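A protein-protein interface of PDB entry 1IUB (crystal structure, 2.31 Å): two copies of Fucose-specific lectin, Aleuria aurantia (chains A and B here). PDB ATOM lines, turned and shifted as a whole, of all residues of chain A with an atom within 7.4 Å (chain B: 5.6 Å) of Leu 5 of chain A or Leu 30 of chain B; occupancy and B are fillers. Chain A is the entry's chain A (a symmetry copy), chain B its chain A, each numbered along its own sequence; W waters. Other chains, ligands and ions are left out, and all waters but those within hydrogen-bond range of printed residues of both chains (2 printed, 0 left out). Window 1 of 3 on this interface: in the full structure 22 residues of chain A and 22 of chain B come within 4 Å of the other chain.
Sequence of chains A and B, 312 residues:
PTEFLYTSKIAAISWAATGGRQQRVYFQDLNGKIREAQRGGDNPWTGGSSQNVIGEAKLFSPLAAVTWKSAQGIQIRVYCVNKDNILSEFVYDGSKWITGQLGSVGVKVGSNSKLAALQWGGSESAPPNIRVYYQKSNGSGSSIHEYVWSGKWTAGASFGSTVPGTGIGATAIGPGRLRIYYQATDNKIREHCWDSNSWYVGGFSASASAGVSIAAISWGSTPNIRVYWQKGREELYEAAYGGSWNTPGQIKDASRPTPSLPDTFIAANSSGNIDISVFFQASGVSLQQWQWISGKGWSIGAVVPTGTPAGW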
ATOM      1  N   THR A   2      21.676  14.289  -7.692  1.00  0.00           N
ATOM      2  CA  THR A   2      23.135  14.279  -7.825  1.00  0.00           C
ATOM      3  C   THR A   2      23.563  12.983  -8.497  1.00  0.00           C
ATOM      4  O   THR A   2      22.724  12.172  -8.893  1.00  0.00           O
ATOM      5  CB  THR A   2      23.838  14.322  -6.454  1.00  0.00           C
ATOM      6  OG1 THR A   2      23.593  13.081  -5.774  1.00  0.00           O
ATOM      7  CG2 THR A   2      23.309  15.482  -5.606  1.00  0.00           C
ATOM      8  N   GLU A   3      24.877  12.780  -8.572  1.00  0.00           N
ATOM      9  CA  GLU A   3      25.439  11.578  -9.174  1.00  0.00           C
ATOM     10  C   GLU A   3      25.898  10.566  -8.134  1.00  0.00           C
ATOM     11  O   GLU A   3      26.562   9.583  -8.456  1.00  0.00           O
ATOM     12  CB  GLU A   3      26.591  11.954 -10.093  1.00  0.00           C
ATOM     13  CG  GLU A   3      26.136  12.883 -11.205  1.00  0.00           C
ATOM     14  CD  GLU A   3      27.274  13.282 -12.149  1.00  0.00           C
ATOM     15  OE1 GLU A   3      28.320  13.799 -11.684  1.00  0.00           O
ATOM     16  OE2 GLU A   3      27.108  13.094 -13.361  1.00  0.00           O
ATOM     17  N   PHE A   4      25.506  10.807  -6.891  1.00  0.00           N
ATOM     18  CA  PHE A   4      25.854   9.945  -5.771  1.00  0.00           C
ATOM     19  C   PHE A   4      24.939   8.727  -5.857  1.00  0.00           C
ATOM     20  O   PHE A   4      23.719   8.853  -5.884  1.00  0.00           O
ATOM     21  CB  PHE A   4      25.625  10.719  -4.456  1.00  0.00           C
ATOM     22  CG  PHE A   4      26.161  10.034  -3.218  1.00  0.00           C
ATOM     23  CD1 PHE A   4      27.019   8.930  -3.310  1.00  0.00           C
ATOM     24  CD2 PHE A   4      25.850  10.541  -1.940  1.00  0.00           C
ATOM     25  CE1 PHE A   4      27.557   8.354  -2.162  1.00  0.00           C
ATOM     26  CE2 PHE A   4      26.387   9.966  -0.783  1.00  0.00           C
ATOM     27  CZ  PHE A   4      27.240   8.872  -0.888  1.00  0.00           C
ATOM     28  N   LEU A   5      25.536   7.548  -5.913  1.00  0.00           N
ATOM     29  CA  LEU A   5      24.770   6.333  -6.004  1.00  0.00           C
ATOM     30  C   LEU A   5      24.090   6.033  -4.654  1.00  0.00           C
ATOM     31  O   LEU A   5      24.752   5.981  -3.615  1.00  0.00           O
ATOM     32  CB  LEU A   5      25.687   5.176  -6.407  1.00  0.00           C
ATOM     33  CG  LEU A   5      25.035   3.789  -6.432  1.00  0.00           C
ATOM     34  CD1 LEU A   5      24.002   3.697  -7.602  1.00  0.00           C
ATOM     35  CD2 LEU A   5      26.106   2.760  -6.588  1.00  0.00           C
ATOM     36  N   TYR A   6      22.778   5.818  -4.678  1.00  0.00           N
ATOM     37  CA  TYR A   6      22.026   5.518  -3.471  1.00  0.00           C
ATOM     38  C   TYR A   6      22.425   4.123  -2.950  1.00  0.00           C
ATOM     39  O   TYR A   6      22.377   3.120  -3.669  1.00  0.00           O
ATOM     40  CB  TYR A   6      20.504   5.609  -3.758  1.00  0.00           C
ATOM     41  CG  TYR A   6      19.624   5.132  -2.619  1.00  0.00           C
ATOM     42  CD1 TYR A   6      19.689   5.729  -1.358  1.00  0.00           C
ATOM     43  CD2 TYR A   6      18.741   4.065  -2.803  1.00  0.00           C
ATOM     44  CE1 TYR A   6      18.894   5.266  -0.302  1.00  0.00           C
ATOM     45  CE2 TYR A   6      17.931   3.605  -1.759  1.00  0.00           C
ATOM     46  CZ  TYR A   6      18.019   4.208  -0.508  1.00  0.00           C
ATOM     47  OH  TYR A   6      17.257   3.731   0.528  1.00  0.00           O
ATOM     48  N   THR A   7      22.812   4.103  -1.679  1.00  0.00           N
ATOM     49  CA  THR A   7      23.305   2.946  -0.929  1.00  0.00           C
ATOM     50  C   THR A   7      24.753   2.608  -1.334  1.00  0.00           C
ATOM     51  O   THR A   7      25.184   1.463  -1.263  1.00  0.00           O
ATOM     52  CB  THR A   7      22.431   1.665  -1.027  1.00  0.00           C
ATOM     53  OG1 THR A   7      22.500   1.103  -2.337  1.00  0.00           O
ATOM     54  CG2 THR A   7      20.987   1.964  -0.653  1.00  0.00           C
ATOM     55  N   SER A   8      25.467   3.627  -1.798  1.00  0.00           N
ATOM     56  CA  SER A   8      26.877   3.524  -2.118  1.00  0.00           C
ATOM     57  C   SER A   8      27.590   3.353  -0.771  1.00  0.00           C
ATOM     58  O   SER A   8      27.145   3.917   0.223  1.00  0.00           O
ATOM     59  CB  SER A   8      27.388   4.831  -2.722  1.00  0.00           C
ATOM     60  OG  SER A   8      28.798   4.869  -2.761  1.00  0.00           O
ATOM     61  N   LYS A   9      28.666   2.577  -0.711  1.00  0.00           N
ATOM     62  CA  LYS A   9      29.383   2.469   0.547  1.00  0.00           C
ATOM     63  C   LYS A   9      30.243   3.713   0.549  1.00  0.00           C
ATOM     64  O   LYS A   9      30.383   4.361  -0.493  1.00  0.00           O
ATOM     65  CB  LYS A   9      30.246   1.209   0.609  1.00  0.00           C
ATOM     66  CG  LYS A   9      29.478  -0.032   1.089  1.00  0.00           C
ATOM     67  CD  LYS A   9      28.536  -0.553  -0.002  1.00  0.00           C
ATOM     68  CE  LYS A   9      28.002  -1.902   0.405  1.00  0.00           C
ATOM     69  NZ  LYS A   9      27.236  -2.576  -0.663  1.00  0.00           N
ATOM     70  N   PHE A  27      33.502   7.694  -2.609  1.00  0.00           N
ATOM     71  CA  PHE A  27      32.136   7.197  -2.760  1.00  0.00           C
ATOM     72  C   PHE A  27      31.925   6.800  -4.214  1.00  0.00           C
ATOM     73  O   PHE A  27      32.728   7.163  -5.084  1.00  0.00           O
ATOM     74  CB  PHE A  27      31.157   8.307  -2.358  1.00  0.00           C
ATOM     75  CG  PHE A  27      31.238   9.532  -3.224  1.00  0.00           C
ATOM     76  CD1 PHE A  27      30.482   9.629  -4.394  1.00  0.00           C
ATOM     77  CD2 PHE A  27      32.042  10.598  -2.854  1.00  0.00           C
ATOM     78  CE1 PHE A  27      30.526  10.776  -5.192  1.00  0.00           C
ATOM     79  CE2 PHE A  27      32.102  11.759  -3.637  1.00  0.00           C
ATOM     80  CZ  PHE A  27      31.340  11.854  -4.811  1.00  0.00           C
ATOM     81  N   GLN A  28      30.850   6.067  -4.492  1.00  0.00           N
ATOM     82  CA  GLN A  28      30.569   5.626  -5.864  1.00  0.00           C
ATOM     83  C   GLN A  28      29.486   6.447  -6.596  1.00  0.00           C
ATOM     84  O   GLN A  28      28.513   6.892  -5.990  1.00  0.00           O
ATOM     85  CB  GLN A  28      30.175   4.148  -5.823  1.00  0.00           C
ATOM     86  CG  GLN A  28      30.214   3.440  -7.170  1.00  0.00           C
ATOM     87  CD  GLN A  28      30.144   1.953  -6.996  1.00  0.00           C
ATOM     88  OE1 GLN A  28      29.370   1.453  -6.179  1.00  0.00           O
ATOM     89  NE2 GLN A  28      30.941   1.223  -7.764  1.00  0.00           N
ATOM     90  N   ASP A  29      29.671   6.690  -7.893  1.00  0.00           N
ATOM     91  CA  ASP A  29      28.668   7.426  -8.649  1.00  0.00           C
ATOM     92  C   ASP A  29      27.717   6.486  -9.419  1.00  0.00           C
ATOM     93  O   ASP A  29      27.834   5.254  -9.339  1.00  0.00           O
ATOM     94  CB  ASP A  29      29.308   8.498  -9.572  1.00  0.00           C
ATOM     95  CG  ASP A  29      30.166   7.924 -10.709  1.00  0.00           C
ATOM     96  OD1 ASP A  29      29.941   6.787 -11.163  1.00  0.00           O
ATOM     97  OD2 ASP A  29      31.065   8.664 -11.179  1.00  0.00           O
ATOM     98  N   LEU A  30      26.749   7.059 -10.119  1.00  0.00           N
ATOM     99  CA  LEU A  30      25.765   6.268 -10.867  1.00  0.00           C
ATOM    100  C   LEU A  30      26.373   5.334 -11.901  1.00  0.00           C
ATOM    101  O   LEU A  30      25.754   4.334 -12.272  1.00  0.00           O
ATOM    102  CB  LEU A  30      24.754   7.196 -11.555  1.00  0.00           C
ATOM    103  CG  LEU A  30      23.925   8.046 -10.590  1.00  0.00           C
ATOM    104  CD1 LEU A  30      23.076   9.040 -11.353  1.00  0.00           C
ATOM    105  CD2 LEU A  30      23.062   7.127  -9.757  1.00  0.00           C
ATOM    106  N   ASN A  31      27.586   5.648 -12.353  1.00  0.00           N
ATOM    107  CA  ASN A  31      28.283   4.824 -13.343  1.00  0.00           C
ATOM    108  C   ASN A  31      29.185   3.763 -12.770  1.00  0.00           C
ATOM    109  O   ASN A  31      29.848   3.067 -13.536  1.00  0.00           O
ATOM    110  CB  ASN A  31      29.130   5.691 -14.258  1.00  0.00           C
ATOM    111  CG  ASN A  31      28.296   6.595 -15.123  1.00  0.00           C
ATOM    112  OD1 ASN A  31      28.527   7.801 -15.161  1.00  0.00           O
ATOM    113  ND2 ASN A  31      27.311   6.024 -15.826  1.00  0.00           N
ATOM    114  N   GLY A  32      29.259   3.648 -11.444  1.00  0.00           N
ATOM    115  CA  GLY A  32      30.120   2.628 -10.855  1.00  0.00           C
ATOM    116  C   GLY A  32      31.552   3.099 -10.590  1.00  0.00           C
ATOM    117  O   GLY A  32      32.364   2.335 -10.087  1.00  0.00           O
ATOM    118  N   LYS A  33      31.848   4.353 -10.917  1.00  0.00           N
ATOM    119  CA  LYS A  33      33.172   4.960 -10.718  1.00  0.00           C
ATOM    120  C   LYS A  33      33.351   5.432  -9.274  1.00  0.00           C
ATOM    121  O   LYS A  33      32.403   5.939  -8.670  1.00  0.00           O
ATOM    122  CB  LYS A  33      33.346   6.189 -11.617  1.00  0.00           C
ATOM    123  CG  LYS A  33      34.024   5.957 -12.939  1.00  0.00           C
ATOM    124  CD  LYS A  33      33.256   5.047 -13.841  1.00  0.00           C
ATOM    125  CE  LYS A  33      34.047   4.840 -15.146  1.00  0.00           C
ATOM    126  NZ  LYS A  33      33.401   3.857 -16.073  1.00  0.00           N
ATOM    127  N   LYS A  58      32.660  -2.739  -9.074  1.00  0.00           N
ATOM    128  CA  LYS A  58      31.317  -3.212  -9.341  1.00  0.00           C
ATOM    129  C   LYS A  58      30.325  -2.240  -8.668  1.00  0.00           C
ATOM    130  O   LYS A  58      30.676  -1.515  -7.734  1.00  0.00           O
ATOM    131  CB  LYS A  58      31.119  -4.624  -8.771  1.00  0.00           C
ATOM    132  CG  LYS A  58      30.823  -4.664  -7.262  1.00  0.00           C
ATOM    133  CD  LYS A  58      30.283  -6.011  -6.881  1.00  0.00           C
ATOM    134  CE  LYS A  58      30.136  -6.218  -5.381  1.00  0.00           C
ATOM    135  NZ  LYS A  58      29.376  -7.516  -5.091  1.00  0.00           N
ATOM    136  N   LEU A  59      29.089  -2.207  -9.154  1.00  0.00           N
ATOM    137  CA  LEU A  59      28.105  -1.315  -8.556  1.00  0.00           C
ATOM    138  C   LEU A  59      27.826  -1.777  -7.131  1.00  0.00           C
ATOM    139  O   LEU A  59      27.668  -2.984  -6.881  1.00  0.00           O
ATOM    140  CB  LEU A  59      26.817  -1.316  -9.393  1.00  0.00           C
ATOM    141  CG  LEU A  59      26.869  -0.408 -10.640  1.00  0.00           C
ATOM    142  CD1 LEU A  59      25.726  -0.739 -11.572  1.00  0.00           C
ATOM    143  CD2 LEU A  59      26.793   1.048 -10.197  1.00  0.00           C
ATOM    144  N   PHE A  60      27.784  -0.829  -6.195  1.00  0.00           N
ATOM    145  CA  PHE A  60      27.489  -1.141  -4.794  1.00  0.00           C
ATOM    146  C   PHE A  60      28.606  -1.887  -4.101  1.00  0.00           C
ATOM    147  O   PHE A  60      28.393  -2.612  -3.128  1.00  0.00           O
ATOM    148  CB  PHE A  60      26.194  -1.948  -4.687  1.00  0.00           C
ATOM    149  CG  PHE A  60      25.035  -1.297  -5.365  1.00  0.00           C
ATOM    150  CD1 PHE A  60      24.525  -1.822  -6.557  1.00  0.00           C
ATOM    151  CD2 PHE A  60      24.474  -0.132  -4.845  1.00  0.00           C
ATOM    152  CE1 PHE A  60      23.462  -1.188  -7.225  1.00  0.00           C
ATOM    153  CE2 PHE A  60      23.414   0.506  -5.506  1.00  0.00           C
ATOM    154  CZ  PHE A  60      22.907  -0.030  -6.707  1.00  0.00           C
ATOM    155  N   SER A  61      29.800  -1.701  -4.638  1.00  0.00           N
ATOM    156  CA  SER A  61      31.000  -2.299  -4.115  1.00  0.00           C
ATOM    157  C   SER A  61      31.340  -1.792  -2.717  1.00  0.00           C
ATOM    158  O   SER A  61      31.146  -0.615  -2.411  1.00  0.00           O
ATOM    159  CB  SER A  61      32.199  -1.947  -5.014  1.00  0.00           C
ATOM    160  OG  SER A  61      33.410  -2.357  -4.397  1.00  0.00           O
ATOM    161  N   THR A 264      21.435   2.850   4.049  1.00  0.00           N
ATOM    162  CA  THR A 264      22.662   3.503   3.671  1.00  0.00           C
ATOM    163  C   THR A 264      23.796   3.115   4.641  1.00  0.00           C
ATOM    164  O   THR A 264      23.579   2.348   5.561  1.00  0.00           O
ATOM    165  CB  THR A 264      22.463   5.007   3.639  1.00  0.00           C
ATOM    166  OG1 THR A 264      22.009   5.437   4.926  1.00  0.00           O
ATOM    167  CG2 THR A 264      21.412   5.378   2.573  1.00  0.00           C
ATOM    168  N   GLN A 281      24.658   9.167   4.186  1.00  0.00           N
ATOM    169  CA  GLN A 281      23.965   9.513   2.943  1.00  0.00           C
ATOM    170  C   GLN A 281      22.542   9.970   3.278  1.00  0.00           C
ATOM    171  O   GLN A 281      21.766   9.241   3.908  1.00  0.00           O
ATOM    172  CB  GLN A 281      23.942   8.289   2.016  1.00  0.00           C
ATOM    173  CG  GLN A 281      23.382   8.588   0.639  1.00  0.00           C
ATOM    174  CD  GLN A 281      23.621   7.465  -0.360  1.00  0.00           C
ATOM    175  OE1 GLN A 281      23.160   6.333  -0.168  1.00  0.00           O
ATOM    176  NE2 GLN A 281      24.332   7.778  -1.437  1.00  0.00           N
ATOM    177  N   VAL A 285      20.335  13.012  -3.739  1.00  0.00           N
ATOM    178  CA  VAL A 285      20.909  12.197  -2.675  1.00  0.00           C
ATOM    179  C   VAL A 285      22.231  12.902  -2.321  1.00  0.00           C
ATOM    180  O   VAL A 285      23.079  13.124  -3.200  1.00  0.00           O
ATOM    181  CB  VAL A 285      21.198  10.796  -3.232  1.00  0.00           C
ATOM    182  CG1 VAL A 285      21.990   9.991  -2.268  1.00  0.00           C
ATOM    183  CG2 VAL A 285      19.890  10.118  -3.566  1.00  0.00           C
ATOM    184  N   THR A 306      28.689  15.981  -4.755  1.00  0.00           N
ATOM    185  CA  THR A 306      28.716  14.677  -5.404  1.00  0.00           C
ATOM    186  C   THR A 306      28.262  14.764  -6.860  1.00  0.00           C
ATOM    187  O   THR A 306      27.736  13.804  -7.408  1.00  0.00           O
ATOM    188  CB  THR A 306      27.805  13.684  -4.661  1.00  0.00           C
ATOM    189  OG1 THR A 306      26.523  14.294  -4.449  1.00  0.00           O
ATOM    190  CG2 THR A 306      28.415  13.284  -3.319  1.00  0.00           C
ATOM    191  N   THR B   2      19.494  -3.614  -7.199  1.00  0.00           N
ATOM    192  CA  THR B   2      18.952  -3.756  -8.554  1.00  0.00           C
ATOM    193  C   THR B   2      19.472  -2.619  -9.418  1.00  0.00           C
ATOM    194  O   THR B   2      20.277  -1.801  -8.967  1.00  0.00           O
ATOM    195  CB  THR B   2      17.414  -3.660  -8.572  1.00  0.00           C
ATOM    196  OG1 THR B   2      17.034  -2.316  -8.240  1.00  0.00           O
ATOM    197  CG2 THR B   2      16.795  -4.629  -7.560  1.00  0.00           C
ATOM    198  N   GLU B   3      18.962  -2.549 -10.647  1.00  0.00           N
ATOM    199  CA  GLU B   3      19.352  -1.505 -11.586  1.00  0.00           C
ATOM    200  C   GLU B   3      18.315  -0.398 -11.688  1.00  0.00           C
ATOM    201  O   GLU B   3      18.389   0.462 -12.563  1.00  0.00           O
ATOM    202  CB  GLU B   3      19.612  -2.117 -12.954  1.00  0.00           C
ATOM    203  CG  GLU B   3      20.720  -3.154 -12.900  1.00  0.00           C
ATOM    204  CD  GLU B   3      21.006  -3.791 -14.264  1.00  0.00           C
ATOM    205  OE1 GLU B   3      20.073  -4.327 -14.911  1.00  0.00           O
ATOM    206  OE2 GLU B   3      22.174  -3.770 -14.674  1.00  0.00           O
ATOM    207  N   PHE B   4      17.368  -0.416 -10.761  1.00  0.00           N
ATOM    208  CA  PHE B   4      16.295   0.567 -10.707  1.00  0.00           C
ATOM    209  C   PHE B   4      16.895   1.837 -10.114  1.00  0.00           C
ATOM    210  O   PHE B   4      17.460   1.821  -9.025  1.00  0.00           O
ATOM    211  CB  PHE B   4      15.161   0.020  -9.815  1.00  0.00           C
ATOM    212  CG  PHE B   4      13.882   0.829  -9.850  1.00  0.00           C
ATOM    213  CD1 PHE B   4      13.677   1.823 -10.815  1.00  0.00           C
ATOM    214  CD2 PHE B   4      12.844   0.546  -8.940  1.00  0.00           C
ATOM    215  CE1 PHE B   4      12.467   2.511 -10.875  1.00  0.00           C
ATOM    216  CE2 PHE B   4      11.626   1.235  -8.996  1.00  0.00           C
ATOM    217  CZ  PHE B   4      11.433   2.219  -9.961  1.00  0.00           C
ATOM    218  N   LEU B   5      16.783   2.936 -10.842  1.00  0.00           N
ATOM    219  CA  LEU B   5      17.322   4.188 -10.381  1.00  0.00           C
ATOM    220  C   LEU B   5      16.459   4.745  -9.232  1.00  0.00           C
ATOM    221  O   LEU B   5      15.241   4.891  -9.373  1.00  0.00           O
ATOM    222  CB  LEU B   5      17.370   5.185 -11.542  1.00  0.00           C
ATOM    223  CG  LEU B   5      17.813   6.606 -11.179  1.00  0.00           C
ATOM    224  CD1 LEU B   5      19.326   6.618 -10.788  1.00  0.00           C
ATOM    225  CD2 LEU B   5      17.560   7.500 -12.350  1.00  0.00           C
ATOM    226  N   TYR B   6      17.093   5.074  -8.110  1.00  0.00           N
ATOM    227  CA  TYR B   6      16.390   5.617  -6.960  1.00  0.00           C
ATOM    228  C   TYR B   6      15.874   7.030  -7.292  1.00  0.00           C
ATOM    229  O   TYR B   6      16.626   7.915  -7.712  1.00  0.00           O
ATOM    230  CB  TYR B   6      17.324   5.623  -5.722  1.00  0.00           C
ATOM    231  CG  TYR B   6      16.756   6.341  -4.513  1.00  0.00           C
ATOM    232  CD1 TYR B   6      15.553   5.934  -3.932  1.00  0.00           C
ATOM    233  CD2 TYR B   6      17.415   7.445  -3.968  1.00  0.00           C
ATOM    234  CE1 TYR B   6      15.018   6.618  -2.833  1.00  0.00           C
ATOM    235  CE2 TYR B   6      16.898   8.127  -2.862  1.00  0.00           C
ATOM    236  CZ  TYR B   6      15.694   7.709  -2.302  1.00  0.00           C
ATOM    237  OH  TYR B   6      15.163   8.401  -1.245  1.00  0.00           O
ATOM    238  N   GLN B  28      13.254   4.120 -15.153  1.00  0.00           N
ATOM    239  CA  GLN B  28      14.638   4.377 -15.569  1.00  0.00           C
ATOM    240  C   GLN B  28      15.702   3.559 -14.807  1.00  0.00           C
ATOM    241  O   GLN B  28      15.564   3.299 -13.614  1.00  0.00           O
ATOM    242  CB  GLN B  28      14.914   5.875 -15.420  1.00  0.00           C
ATOM    243  CG  GLN B  28      16.157   6.369 -16.148  1.00  0.00           C
ATOM    244  CD  GLN B  28      16.170   7.866 -16.230  1.00  0.00           C
ATOM    245  OE1 GLN B  28      15.841   8.549 -15.259  1.00  0.00           O
ATOM    246  NE2 GLN B  28      16.556   8.399 -17.380  1.00  0.00           N
ATOM    247  N   ASP B  29      16.746   3.112 -15.502  1.00  0.00           N
ATOM    248  CA  ASP B  29      17.804   2.367 -14.834  1.00  0.00           C
ATOM    249  C   ASP B  29      19.004   3.265 -14.466  1.00  0.00           C
ATOM    250  O   ASP B  29      18.992   4.479 -14.717  1.00  0.00           O
ATOM    251  CB  ASP B  29      18.235   1.116 -15.647  1.00  0.00           C
ATOM    252  CG  ASP B  29      18.908   1.435 -16.991  1.00  0.00           C
ATOM    253  OD1 ASP B  29      19.517   2.508 -17.157  1.00  0.00           O
ATOM    254  OD2 ASP B  29      18.851   0.555 -17.885  1.00  0.00           O
ATOM    255  N   LEU B  30      20.010   2.685 -13.828  1.00  0.00           N
ATOM    256  CA  LEU B  30      21.192   3.443 -13.400  1.00  0.00           C
ATOM    257  C   LEU B  30      21.919   4.155 -14.530  1.00  0.00           C
ATOM    258  O   LEU B  30      22.619   5.141 -14.290  1.00  0.00           O
ATOM    259  CB  LEU B  30      22.175   2.520 -12.667  1.00  0.00           C
ATOM    260  CG  LEU B  30      21.616   1.901 -11.383  1.00  0.00           C
ATOM    261  CD1 LEU B  30      22.586   0.887 -10.817  1.00  0.00           C
ATOM    262  CD2 LEU B  30      21.351   3.007 -10.390  1.00  0.00           C
ATOM    263  N   ASN B  31      21.742   3.669 -15.757  1.00  0.00           N
ATOM    264  CA  ASN B  31      22.381   4.270 -16.929  1.00  0.00           C
ATOM    265  C   ASN B  31      21.560   5.318 -17.637  1.00  0.00           C
ATOM    266  O   ASN B  31      22.003   5.829 -18.663  1.00  0.00           O
ATOM    267  CB  ASN B  31      22.729   3.204 -17.953  1.00  0.00           C
ATOM    268  CG  ASN B  31      23.792   2.261 -17.458  1.00  0.00           C
ATOM    269  OD1 ASN B  31      23.611   1.047 -17.501  1.00  0.00           O
ATOM    270  ND2 ASN B  31      24.913   2.810 -16.976  1.00  0.00           N
ATOM    271  N   GLY B  32      20.361   5.619 -17.139  1.00  0.00           N
ATOM    272  CA  GLY B  32      19.542   6.633 -17.796  1.00  0.00           C
ATOM    273  C   GLY B  32      18.615   6.078 -18.881  1.00  0.00           C
ATOM    274  O   GLY B  32      17.872   6.831 -19.494  1.00  0.00           O
ATOM    275  N   LEU B  59      18.940  11.740 -16.852  1.00  0.00           N
ATOM    276  CA  LEU B  59      18.774  11.039 -15.586  1.00  0.00           C
ATOM    277  C   LEU B  59      17.677  11.731 -14.784  1.00  0.00           C
ATOM    278  O   LEU B  59      17.637  12.971 -14.712  1.00  0.00           O
ATOM    279  CB  LEU B  59      20.099  11.035 -14.810  1.00  0.00           C
ATOM    280  CG  LEU B  59      21.099   9.951 -15.267  1.00  0.00           C
ATOM    281  CD1 LEU B  59      22.472  10.244 -14.709  1.00  0.00           C
ATOM    282  CD2 LEU B  59      20.607   8.591 -14.790  1.00  0.00           C
ATOM    283  N   PRO B 309      22.624  -5.918 -11.011  1.00  0.00           N
ATOM    284  CA  PRO B 309      23.938  -5.522 -11.534  1.00  0.00           C
ATOM    285  C   PRO B 309      24.948  -6.663 -11.499  1.00  0.00           C
ATOM    286  O   PRO B 309      24.828  -7.619 -10.714  1.00  0.00           O
ATOM    287  CB  PRO B 309      24.333  -4.340 -10.632  1.00  0.00           C
ATOM    288  CG  PRO B 309      23.678  -4.662  -9.348  1.00  0.00           C
ATOM    289  CD  PRO B 309      22.316  -5.216  -9.750  1.00  0.00           C
HETATM  290  O   HOH W   1      25.628   2.224 -14.114  1.00  0.00           O
HETATM  291  O   HOH W   2      24.502   6.960 -15.296  1.00  0.00           O
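N of Phe 4 of chain B is in hydrogen-bond range of OG1 of Thr 2 of chain B (3.2 Å). The backbone carbonyl oxygen (O) of Glu 3 of chain B lies within hydrogen-bond range of the backbone NH (N) of Leu 30 of chain B. N of Leu 5 of chain B is in hydrogen-bond range of O of Gln 28 of chain B, 3.0 Å away. The backbone carbonyl oxygen (O) of Leu 5 of chain A is in hydrogen-bond range of the side-chain amide nitrogen (NE2) of Gln 281 of chain A, 2.9 Å away. O of Phe 60 of chain A is in hydrogen-bond range of NZ of Lys 9 of chain A, 2.7 Å away. The backbone NH of Phe 60 of chain A sits at hydrogen-bond distance from the side-chain amide oxygen of Gln 28 of chain A, 2.8 Å away.
Leu 5 of chain A touches just one residue of chain B: Leu 30 (3.9 Å). Lys 9 of chain A touches none of the printed residues of chain B. Of the printed residues of chain B, Leu 30 of chain A touches Leu 5, Leu 30 and Leu 59. Of the printed residues of chain B, Phe 60 of chain A touches Thr 2. Of the printed residues of chain A, Tyr 6 of chain B touches Tyr 6 and Val 285. Leu 30 of chain B touches just these residues of chain A: Leu 5, Leu 30 and Leu 59. The nearest printed residue of chain B that does not touch Tyr 6 of chain A is Leu 30 of chain B (6.5 Å).
Leu 5 of chain A touches Leu 30 of chain B, and with the chains exchanged Leu 30 of chain A touches Leu 5 of chain B. Tyr 6 of chain B touches its own counterpart, Tyr 6 of chain A. Leu 30 of chain B touches its own counterpart, Leu 30 of chain A. Leu 30 of chain A touches Leu 59 of chain B, and with the chains exchanged Leu 59 of chain A touches Leu 30 of chain B. Of the 9 pairs that touch across the chains among the printed residues, 6 have their exchanged pair printed and touching as well.
Water W1 lies within hydrogen-bond range of the backbone carbonyl oxygen (O) of Leu 30 of chain A and the side-chain amide nitrogen (ND2) of Asn 31 of chain B. Water W2 lies within hydrogen-bond range of the backbone carbonyl oxygen (O) of Leu 30 of chain B and the side-chain amide nitrogen (ND2) of Asn 31 of chain A.
Hydrophobic or aromatic side chains of chain A that line the printed part of chain B: Leu 5, Tyr 6, Leu 30, Leu 59, Phe 60 and Val 285. Of the 12 printed residues of chain B, 6 touch a printed residue of chain A. Printed residues of chain B that touch a printed residue of chain A: Thr 2, Leu 5, Tyr 6, Leu 30, Leu 59 and Pro 309. Hydrophobic or aromatic side chains of chain B within 4 Å of the printed part of chain A: Leu 5, Tyr 6, Leu 30, Leu 59 and Pro 309. Along chain B the printed residues that touch a printed residue of chain A span positions 2 to 309. Among the printed residues, no Asp or Glu carboxylate lies within 4 Å of a Lys or Arg side-chain nitrogen of the other chain.
CD1 of Leu 5 of chain A touches CD2 of Leu 30 of chain B (3.9 Å). CG of Tyr 6 of chain B touches CD2 of Tyr 6 of chain A (3.5 Å). Leu 30 of chain A touches Leu 5 of chain B (CD2 to CD1, 3.9 Å). Leu 30 of chain A touches Leu 30 of chain B. CD1 of Leu 59 of chain B touches CD1 of Leu 30 of chain A, 3.6 Å away. Leu 30 of chain B touches Leu 59 of chain A. CD1 of Leu 59 of chain A touches CB of Pro 309 of chain B, at 3.97 Å. Thr 2 of chain B touches Phe 60 of chain A. Tyr 6 of chain B touches Val 285 of chain A.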
